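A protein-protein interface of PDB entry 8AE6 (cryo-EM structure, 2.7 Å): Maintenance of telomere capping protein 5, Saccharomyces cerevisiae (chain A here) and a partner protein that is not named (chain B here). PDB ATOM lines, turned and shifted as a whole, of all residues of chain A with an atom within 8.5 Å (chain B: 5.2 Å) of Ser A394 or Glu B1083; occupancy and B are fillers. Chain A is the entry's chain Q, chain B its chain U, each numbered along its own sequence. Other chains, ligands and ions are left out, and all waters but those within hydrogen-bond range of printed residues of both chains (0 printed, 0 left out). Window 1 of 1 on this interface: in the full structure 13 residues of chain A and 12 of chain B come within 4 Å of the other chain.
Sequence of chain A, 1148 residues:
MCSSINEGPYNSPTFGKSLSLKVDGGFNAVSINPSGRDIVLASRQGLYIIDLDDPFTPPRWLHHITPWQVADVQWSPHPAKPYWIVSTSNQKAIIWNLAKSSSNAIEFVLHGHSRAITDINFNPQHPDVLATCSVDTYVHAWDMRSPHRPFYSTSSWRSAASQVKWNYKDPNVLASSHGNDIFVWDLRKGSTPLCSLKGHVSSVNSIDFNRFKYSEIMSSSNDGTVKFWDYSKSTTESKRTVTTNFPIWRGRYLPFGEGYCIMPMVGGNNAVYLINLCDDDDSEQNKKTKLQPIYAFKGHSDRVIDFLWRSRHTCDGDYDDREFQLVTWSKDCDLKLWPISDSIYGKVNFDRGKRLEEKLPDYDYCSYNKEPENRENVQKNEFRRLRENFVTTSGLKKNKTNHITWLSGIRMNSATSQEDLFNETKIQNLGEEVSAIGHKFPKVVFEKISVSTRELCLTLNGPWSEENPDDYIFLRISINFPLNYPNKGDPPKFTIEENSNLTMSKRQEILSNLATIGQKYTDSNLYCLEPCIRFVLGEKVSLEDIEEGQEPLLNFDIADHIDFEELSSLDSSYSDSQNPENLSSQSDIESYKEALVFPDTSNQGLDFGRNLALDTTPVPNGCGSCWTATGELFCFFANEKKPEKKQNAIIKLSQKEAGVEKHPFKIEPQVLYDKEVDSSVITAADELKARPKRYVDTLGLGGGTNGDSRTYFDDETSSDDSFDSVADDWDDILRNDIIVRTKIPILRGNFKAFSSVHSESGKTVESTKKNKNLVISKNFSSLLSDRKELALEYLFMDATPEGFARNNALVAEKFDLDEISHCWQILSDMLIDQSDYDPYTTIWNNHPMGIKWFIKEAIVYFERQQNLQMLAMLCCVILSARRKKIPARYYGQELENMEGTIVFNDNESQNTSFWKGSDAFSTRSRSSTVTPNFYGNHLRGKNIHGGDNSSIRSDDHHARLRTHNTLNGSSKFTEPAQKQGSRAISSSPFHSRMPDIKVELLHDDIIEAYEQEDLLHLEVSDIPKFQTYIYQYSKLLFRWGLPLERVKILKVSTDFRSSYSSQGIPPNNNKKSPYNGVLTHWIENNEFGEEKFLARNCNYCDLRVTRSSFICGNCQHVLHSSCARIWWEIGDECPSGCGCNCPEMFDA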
ATOM      1  N   ASN A 389       1.109  20.797   7.386  1.00  0.00           N
ATOM      2  CA  ASN A 389       2.275  21.661   7.533  1.00  0.00           C
ATOM      3  C   ASN A 389       3.376  20.997   6.720  1.00  0.00           C
ATOM      4  O   ASN A 389       4.090  20.123   7.208  1.00  0.00           O
ATOM      5  CB  ASN A 389       2.667  21.830   8.994  1.00  0.00           C
ATOM      6  CG  ASN A 389       3.680  22.935   9.197  1.00  0.00           C
ATOM      7  OD1 ASN A 389       3.873  23.780   8.326  1.00  0.00           O
ATOM      8  ND2 ASN A 389       4.333  22.934  10.352  1.00  0.00           N
ATOM      9  N   VAL A 391       6.254  22.240   4.808  1.00  0.00           N
ATOM     10  CA  VAL A 391       7.628  22.627   5.081  1.00  0.00           C
ATOM     11  C   VAL A 391       7.601  23.649   6.206  1.00  0.00           C
ATOM     12  O   VAL A 391       6.614  24.372   6.379  1.00  0.00           O
ATOM     13  CB  VAL A 391       8.319  23.172   3.806  1.00  0.00           C
ATOM     14  CG1 VAL A 391       7.719  24.502   3.358  1.00  0.00           C
ATOM     15  CG2 VAL A 391       9.830  23.262   3.974  1.00  0.00           C
ATOM     16  N   THR A 392       8.656  23.663   7.011  1.00  0.00           N
ATOM     17  CA  THR A 392       8.741  24.594   8.123  1.00  0.00           C
ATOM     18  C   THR A 392       8.912  26.022   7.616  1.00  0.00           C
ATOM     19  O   THR A 392       9.730  26.293   6.735  1.00  0.00           O
ATOM     20  CB  THR A 392       9.906  24.214   9.033  1.00  0.00           C
ATOM     21  OG1 THR A 392       9.787  22.837   9.402  1.00  0.00           O
ATOM     22  CG2 THR A 392       9.901  25.064  10.276  1.00  0.00           C
ATOM     23  N   THR A 393       8.117  26.935   8.181  1.00  0.00           N
ATOM     24  CA  THR A 393       8.208  28.343   7.812  1.00  0.00           C
ATOM     25  C   THR A 393       9.524  28.955   8.284  1.00  0.00           C
ATOM     26  O   THR A 393      10.092  29.812   7.593  1.00  0.00           O
ATOM     27  CB  THR A 393       7.003  29.098   8.388  1.00  0.00           C
ATOM     28  OG1 THR A 393       5.798  28.527   7.869  1.00  0.00           O
ATOM     29  CG2 THR A 393       7.029  30.577   8.012  1.00  0.00           C
ATOM     30  N   SER A 394      10.048  28.493   9.424  1.00  0.00           N
ATOM     31  CA  SER A 394      11.293  29.039   9.957  1.00  0.00           C
ATOM     32  C   SER A 394      12.497  28.698   9.092  1.00  0.00           C
ATOM     33  O   SER A 394      13.510  29.403   9.161  1.00  0.00           O
ATOM     34  CB  SER A 394      11.526  28.535  11.378  1.00  0.00           C
ATOM     35  OG  SER A 394      12.099  27.240  11.372  1.00  0.00           O
ATOM     36  N   GLY A 395      12.417  27.646   8.286  1.00  0.00           N
ATOM     37  CA  GLY A 395      13.477  27.331   7.354  1.00  0.00           C
ATOM     38  C   GLY A 395      13.441  28.104   6.060  1.00  0.00           C
ATOM     39  O   GLY A 395      14.360  27.976   5.245  1.00  0.00           O
ATOM     40  N   LEU A 396      12.407  28.907   5.842  1.00  0.00           N
ATOM     41  CA  LEU A 396      12.286  29.693   4.620  1.00  0.00           C
ATOM     42  C   LEU A 396      12.976  31.044   4.773  1.00  0.00           C
ATOM     43  O   LEU A 396      12.591  32.021   4.131  1.00  0.00           O
ATOM     44  CB  LEU A 396      10.811  29.893   4.257  1.00  0.00           C
ATOM     45  CG  LEU A 396       9.993  28.625   4.008  1.00  0.00           C
ATOM     46  CD1 LEU A 396       8.520  28.958   3.865  1.00  0.00           C
ATOM     47  CD2 LEU A 396      10.498  27.910   2.771  1.00  0.00           C
ATOM     48  N   GLU A 447      14.965  37.986  13.231  1.00  0.00           N
ATOM     49  CA  GLU A 447      13.792  37.241  12.788  1.00  0.00           C
ATOM     50  C   GLU A 447      12.512  38.061  12.845  1.00  0.00           C
ATOM     51  O   GLU A 447      11.611  37.845  12.027  1.00  0.00           O
ATOM     52  CB  GLU A 447      13.622  35.970  13.621  1.00  0.00           C
ATOM     53  CG  GLU A 447      14.263  34.741  13.002  1.00  0.00           C
ATOM     54  CD  GLU A 447      13.766  33.448  13.620  1.00  0.00           C
ATOM     55  OE1 GLU A 447      13.018  33.515  14.617  1.00  0.00           O
ATOM     56  OE2 GLU A 447      14.125  32.367  13.107  1.00  0.00           O
ATOM     57  N   THR A 459      18.170  36.029  16.342  1.00  0.00           N
ATOM     58  CA  THR A 459      18.837  34.740  16.446  1.00  0.00           C
ATOM     59  C   THR A 459      20.332  34.917  16.229  1.00  0.00           C
ATOM     60  O   THR A 459      20.755  35.705  15.377  1.00  0.00           O
ATOM     61  CB  THR A 459      18.287  33.756  15.416  1.00  0.00           C
ATOM     62  OG1 THR A 459      18.598  34.222  14.098  1.00  0.00           O
ATOM     63  CG2 THR A 459      16.783  33.643  15.540  1.00  0.00           C
ATOM     64  N   PHE A 474      23.159  27.806  18.883  1.00  0.00           N
ATOM     65  CA  PHE A 474      22.103  28.643  18.327  1.00  0.00           C
ATOM     66  C   PHE A 474      21.149  29.066  19.437  1.00  0.00           C
ATOM     67  O   PHE A 474      20.611  28.221  20.160  1.00  0.00           O
ATOM     68  CB  PHE A 474      21.351  27.886  17.238  1.00  0.00           C
ATOM     69  CG  PHE A 474      20.608  28.773  16.284  1.00  0.00           C
ATOM     70  CD1 PHE A 474      19.308  29.162  16.549  1.00  0.00           C
ATOM     71  CD2 PHE A 474      21.213  29.213  15.120  1.00  0.00           C
ATOM     72  CE1 PHE A 474      18.626  29.975  15.671  1.00  0.00           C
ATOM     73  CE2 PHE A 474      20.536  30.027  14.237  1.00  0.00           C
ATOM     74  CZ  PHE A 474      19.240  30.407  14.514  1.00  0.00           C
ATOM     75  N   ARG A 476      17.810  31.735  20.512  1.00  0.00           N
ATOM     76  CA  ARG A 476      16.723  32.630  20.138  1.00  0.00           C
ATOM     77  C   ARG A 476      16.363  33.480  21.347  1.00  0.00           C
ATOM     78  O   ARG A 476      15.897  32.954  22.362  1.00  0.00           O
ATOM     79  CB  ARG A 476      15.504  31.854  19.650  1.00  0.00           C
ATOM     80  CG  ARG A 476      15.574  31.441  18.199  1.00  0.00           C
ATOM     81  CD  ARG A 476      14.220  31.575  17.527  1.00  0.00           C
ATOM     82  NE  ARG A 476      14.290  31.289  16.102  1.00  0.00           N
ATOM     83  CZ  ARG A 476      14.140  30.082  15.573  1.00  0.00           C
ATOM     84  NH1 ARG A 476      13.912  29.020  16.327  1.00  0.00           N
ATOM     85  NH2 ARG A 476      14.219  29.938  14.254  1.00  0.00           N
ATOM     86  N   GLU A 497      14.261  31.671  24.214  1.00  0.00           N
ATOM     87  CA  GLU A 497      13.503  30.481  23.854  1.00  0.00           C
ATOM     88  C   GLU A 497      14.114  29.245  24.507  1.00  0.00           C
ATOM     89  O   GLU A 497      15.333  29.159  24.686  1.00  0.00           O
ATOM     90  CB  GLU A 497      13.468  30.326  22.331  1.00  0.00           C
ATOM     91  CG  GLU A 497      12.547  29.237  21.815  1.00  0.00           C
ATOM     92  CD  GLU A 497      12.245  29.380  20.339  1.00  0.00           C
ATOM     93  OE1 GLU A 497      12.095  30.527  19.872  1.00  0.00           O
ATOM     94  OE2 GLU A 497      12.160  28.347  19.646  1.00  0.00           O
ATOM     95  N   ILE B1073      11.378  19.541   7.956  1.00  0.00           N
ATOM     96  CA  ILE B1073      12.139  20.586   8.630  1.00  0.00           C
ATOM     97  C   ILE B1073      13.264  21.003   7.692  1.00  0.00           C
ATOM     98  O   ILE B1073      14.215  20.249   7.471  1.00  0.00           O
ATOM     99  CB  ILE B1073      12.676  20.114   9.982  1.00  0.00           C
ATOM    100  CG1 ILE B1073      11.514  19.696  10.879  1.00  0.00           C
ATOM    101  CG2 ILE B1073      13.485  21.212  10.645  1.00  0.00           C
ATOM    102  CD1 ILE B1073      11.936  19.090  12.188  1.00  0.00           C
ATOM    103  N   ARG B1078      18.297  26.069  12.595  1.00  0.00           N
ATOM    104  CA  ARG B1078      17.407  27.121  13.088  1.00  0.00           C
ATOM    105  C   ARG B1078      15.979  26.599  13.243  1.00  0.00           C
ATOM    106  O   ARG B1078      15.012  27.131  12.697  1.00  0.00           O
ATOM    107  CB  ARG B1078      17.475  28.342  12.172  1.00  0.00           C
ATOM    108  CG  ARG B1078      17.291  28.059  10.694  1.00  0.00           C
ATOM    109  CD  ARG B1078      17.419  29.324   9.867  1.00  0.00           C
ATOM    110  NE  ARG B1078      18.790  29.822   9.834  1.00  0.00           N
ATOM    111  CZ  ARG B1078      19.205  30.915  10.458  1.00  0.00           C
ATOM    112  NH1 ARG B1078      18.378  31.654  11.180  1.00  0.00           N
ATOM    113  NH2 ARG B1078      20.480  31.278  10.354  1.00  0.00           N
ATOM    114  N   ALA B1079      15.852  25.540  14.029  1.00  0.00           N
ATOM    115  CA  ALA B1079      14.559  24.962  14.347  1.00  0.00           C
ATOM    116  C   ALA B1079      14.008  25.577  15.627  1.00  0.00           C
ATOM    117  O   ALA B1079      14.754  26.049  16.490  1.00  0.00           O
ATOM    118  CB  ALA B1079      14.661  23.443  14.492  1.00  0.00           C
ATOM    119  N   THR B1080      12.684  25.564  15.744  1.00  0.00           N
ATOM    120  CA  THR B1080      12.014  26.125  16.908  1.00  0.00           C
ATOM    121  C   THR B1080      12.041  25.113  18.051  1.00  0.00           C
ATOM    122  O   THR B1080      12.714  24.079  17.986  1.00  0.00           O
ATOM    123  CB  THR B1080      10.591  26.544  16.555  1.00  0.00           C
ATOM    124  OG1 THR B1080       9.773  25.380  16.404  1.00  0.00           O
ATOM    125  CG2 THR B1080      10.574  27.342  15.262  1.00  0.00           C
ATOM    126  N   ALA B1081      11.307  25.410  19.125  1.00  0.00           N
ATOM    127  CA  ALA B1081      11.301  24.522  20.283  1.00  0.00           C
ATOM    128  C   ALA B1081      10.559  23.226  19.987  1.00  0.00           C
ATOM    129  O   ALA B1081      11.001  22.147  20.396  1.00  0.00           O
ATOM    130  CB  ALA B1081      10.679  25.233  21.483  1.00  0.00           C
ATOM    131  N   ILE B1082       9.429  23.313  19.282  1.00  0.00           N
ATOM    132  CA  ILE B1082       8.662  22.113  18.968  1.00  0.00           C
ATOM    133  C   ILE B1082       9.359  21.283  17.893  1.00  0.00           C
ATOM    134  O   ILE B1082       9.308  20.047  17.923  1.00  0.00           O
ATOM    135  CB  ILE B1082       7.218  22.501  18.583  1.00  0.00           C
ATOM    136  CG1 ILE B1082       6.356  21.265  18.321  1.00  0.00           C
ATOM    137  CG2 ILE B1082       7.183  23.469  17.403  1.00  0.00           C
ATOM    138  CD1 ILE B1082       4.883  21.568  18.164  1.00  0.00           C
ATOM    139  N   GLU B1083      10.049  21.930  16.951  1.00  0.00           N
ATOM    140  CA  GLU B1083      10.671  21.204  15.850  1.00  0.00           C
ATOM    141  C   GLU B1083      11.961  20.513  16.272  1.00  0.00           C
ATOM    142  O   GLU B1083      12.283  19.439  15.756  1.00  0.00           O
ATOM    143  CB  GLU B1083      10.925  22.151  14.683  1.00  0.00           C
ATOM    144  CG  GLU B1083       9.661  22.576  13.975  1.00  0.00           C
ATOM    145  CD  GLU B1083       9.685  24.031  13.583  1.00  0.00           C
ATOM    146  OE1 GLU B1083      10.794  24.585  13.440  1.00  0.00           O
ATOM    147  OE2 GLU B1083       8.598  24.622  13.415  1.00  0.00           O
ATOM    148  N   LYS B1084      12.723  21.118  17.184  1.00  0.00           N
ATOM    149  CA  LYS B1084      13.889  20.430  17.726  1.00  0.00           C
ATOM    150  C   LYS B1084      13.479  19.234  18.572  1.00  0.00           C
ATOM    151  O   LYS B1084      14.237  18.263  18.683  1.00  0.00           O
ATOM    152  CB  LYS B1084      14.743  21.393  18.549  1.00  0.00           C
ATOM    153  CG  LYS B1084      15.862  22.051  17.763  1.00  0.00           C
ATOM    154  CD  LYS B1084      16.563  23.115  18.587  1.00  0.00           C
ATOM    155  CE  LYS B1084      17.681  23.777  17.799  1.00  0.00           C
ATOM    156  NZ  LYS B1084      17.155  24.718  16.773  1.00  0.00           N
ATOM    157  N   ARG B1085      12.292  19.289  19.176  1.00  0.00           N
ATOM    158  CA  ARG B1085      11.744  18.116  19.844  1.00  0.00           C
ATOM    159  C   ARG B1085      11.361  17.045  18.833  1.00  0.00           C
ATOM    160  O   ARG B1085      11.445  15.848  19.125  1.00  0.00           O
ATOM    161  CB  ARG B1085      10.536  18.516  20.689  1.00  0.00           C
ATOM    162  CG  ARG B1085      10.900  19.186  21.996  1.00  0.00           C
ATOM    163  CD  ARG B1085       9.739  19.163  22.965  1.00  0.00           C
ATOM    164  NE  ARG B1085       9.884  20.173  24.004  1.00  0.00           N
ATOM    165  CZ  ARG B1085       9.435  20.042  25.244  1.00  0.00           C
ATOM    166  NH1 ARG B1085       8.803  18.949  25.638  1.00  0.00           N
ATOM    167  NH2 ARG B1085       9.625  21.033  26.113  1.00  0.00           N
ATOM    168  N   TRP B1086      10.921  17.461  17.641  1.00  0.00           N
ATOM    169  CA  TRP B1086      10.615  16.503  16.584  1.00  0.00           C
ATOM    170  C   TRP B1086      11.873  15.797  16.092  1.00  0.00           C
ATOM    171  O   TRP B1086      11.846  14.596  15.803  1.00  0.00           O
ATOM    172  CB  TRP B1086       9.917  17.206  15.417  1.00  0.00           C
ATOM    173  CG  TRP B1086       8.544  17.695  15.718  1.00  0.00           C
ATOM    174  CD1 TRP B1086       7.769  17.360  16.783  1.00  0.00           C
ATOM    175  CD2 TRP B1086       7.771  18.612  14.936  1.00  0.00           C
ATOM    176  NE1 TRP B1086       6.563  18.010  16.718  1.00  0.00           N
ATOM    177  CE2 TRP B1086       6.542  18.787  15.591  1.00  0.00           C
ATOM    178  CE3 TRP B1086       8.003  19.303  13.745  1.00  0.00           C
ATOM    179  CZ2 TRP B1086       5.545  19.622  15.098  1.00  0.00           C
ATOM    180  CZ3 TRP B1086       7.014  20.131  13.256  1.00  0.00           C
ATOM    181  CH2 TRP B1086       5.800  20.283  13.931  1.00  0.00           C
ATOM    182  N   LEU B1087      12.978  16.536  15.971  1.00  0.00           N
ATOM    183  CA  LEU B1087      14.229  15.944  15.510  1.00  0.00           C
ATOM    184  C   LEU B1087      14.777  14.953  16.523  1.00  0.00           C
ATOM    185  O   LEU B1087      15.268  13.881  16.150  1.00  0.00           O
ATOM    186  CB  LEU B1087      15.260  17.039  15.241  1.00  0.00           C
ATOM    187  CG  LEU B1087      14.941  18.063  14.158  1.00  0.00           C
ATOM    188  CD1 LEU B1087      15.671  19.366  14.428  1.00  0.00           C
ATOM    189  CD2 LEU B1087      15.315  17.518  12.802  1.00  0.00           C
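Of the 12 printed residues of chain A, 6 touch a printed residue of chain B. Hydrophobic or aromatic side chains of chain A that line the printed part of chain B: Phe A474. Of the 11 printed residues of chain B, 6 touch a printed residue of chain A. Hydrophobic or aromatic side chains of chain B that line the printed part of chain A: Ile B1073 and Ala B1081.
The side-chain amino group of Lys B1084 is in hydrogen-bond range of the backbone carbonyl oxygen of Ala B1079 (2.8 Å). N of Thr B1080 is in hydrogen-bond range of OE1 of Glu B1083, at 3.1 Å. The side-chain carboxylate (OE2) of Glu A447 is in salt-bridge range of the guanidinium group (NH2) of Arg A476, 2.7 Å away. OE2 of Glu A497 lies within salt-bridge range of NH1 of Arg A476.
Ile B1073 touches Thr A392 (CA to OG1, 3.3 Å). OE1 of Glu B1083 touches CG2 of Thr A392, 3.3 Å away. OE1 of Glu B1083 touches OG of Ser A394 (3.6 Å). OG1 of Thr A459 touches NH1 of Arg B1078 (3.9 Å). CZ of Phe A474 touches CB of Arg B1078, at 3.6 Å. Arg A476 touches Thr B1080. Glu A497 touches Thr B1080 (OE2 to CA, 3.5 Å).
The backbone carbonyl oxygen (O) of Arg B1078 sits at hydrogen-bond distance from the side-chain hydroxyl (OG) of Ser A394 (3.2 Å). The guanidinium group (NH2) of Arg A476 sits at hydrogen-bond distance from the backbone carbonyl oxygen (O) of Arg B1078. The backbone carbonyl oxygen (O) of Ala B1079 sits at hydrogen-bond distance from the guanidinium group (NH1) of Arg A476, at 3.1 Å. The side-chain carboxylate (OE2) of Glu A497 is in hydrogen-bond range of the backbone NH (N) of Ala B1081 (3.1 Å).
Ser A394 touches just these residues of chain B: Arg B1078 (3.2 Å) and Glu B1083 (3.6 Å). Of chain A, only Arg A476 and Glu A497 come within 4 Å of Thr B1080. Printed residues of chain A within 4 Å of Arg B1078: Ser A394 (3.2 Å), Thr A459 (3.9 Å), Phe A474 (3.6 Å) and Arg A476 (3.3 Å). Of the printed residues of chain A, Ile B1073 touches Thr A392 (3.3 Å). Printed residues of chain A within 4 Å of Ala B1079: Arg A476. Of the printed residues of chain A, Ala B1081 touches Glu A497. Of the printed residues of chain B, Arg A476 touches Arg B1078, Ala B1079 and Thr B1080. Val A391 touches none of the printed residues of chain B. Ile B1082 touches none of the printed residues of chain A. The nearest printed residue of chain B that does not touch Glu A497 is Ala B1079 (4.7 Å).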
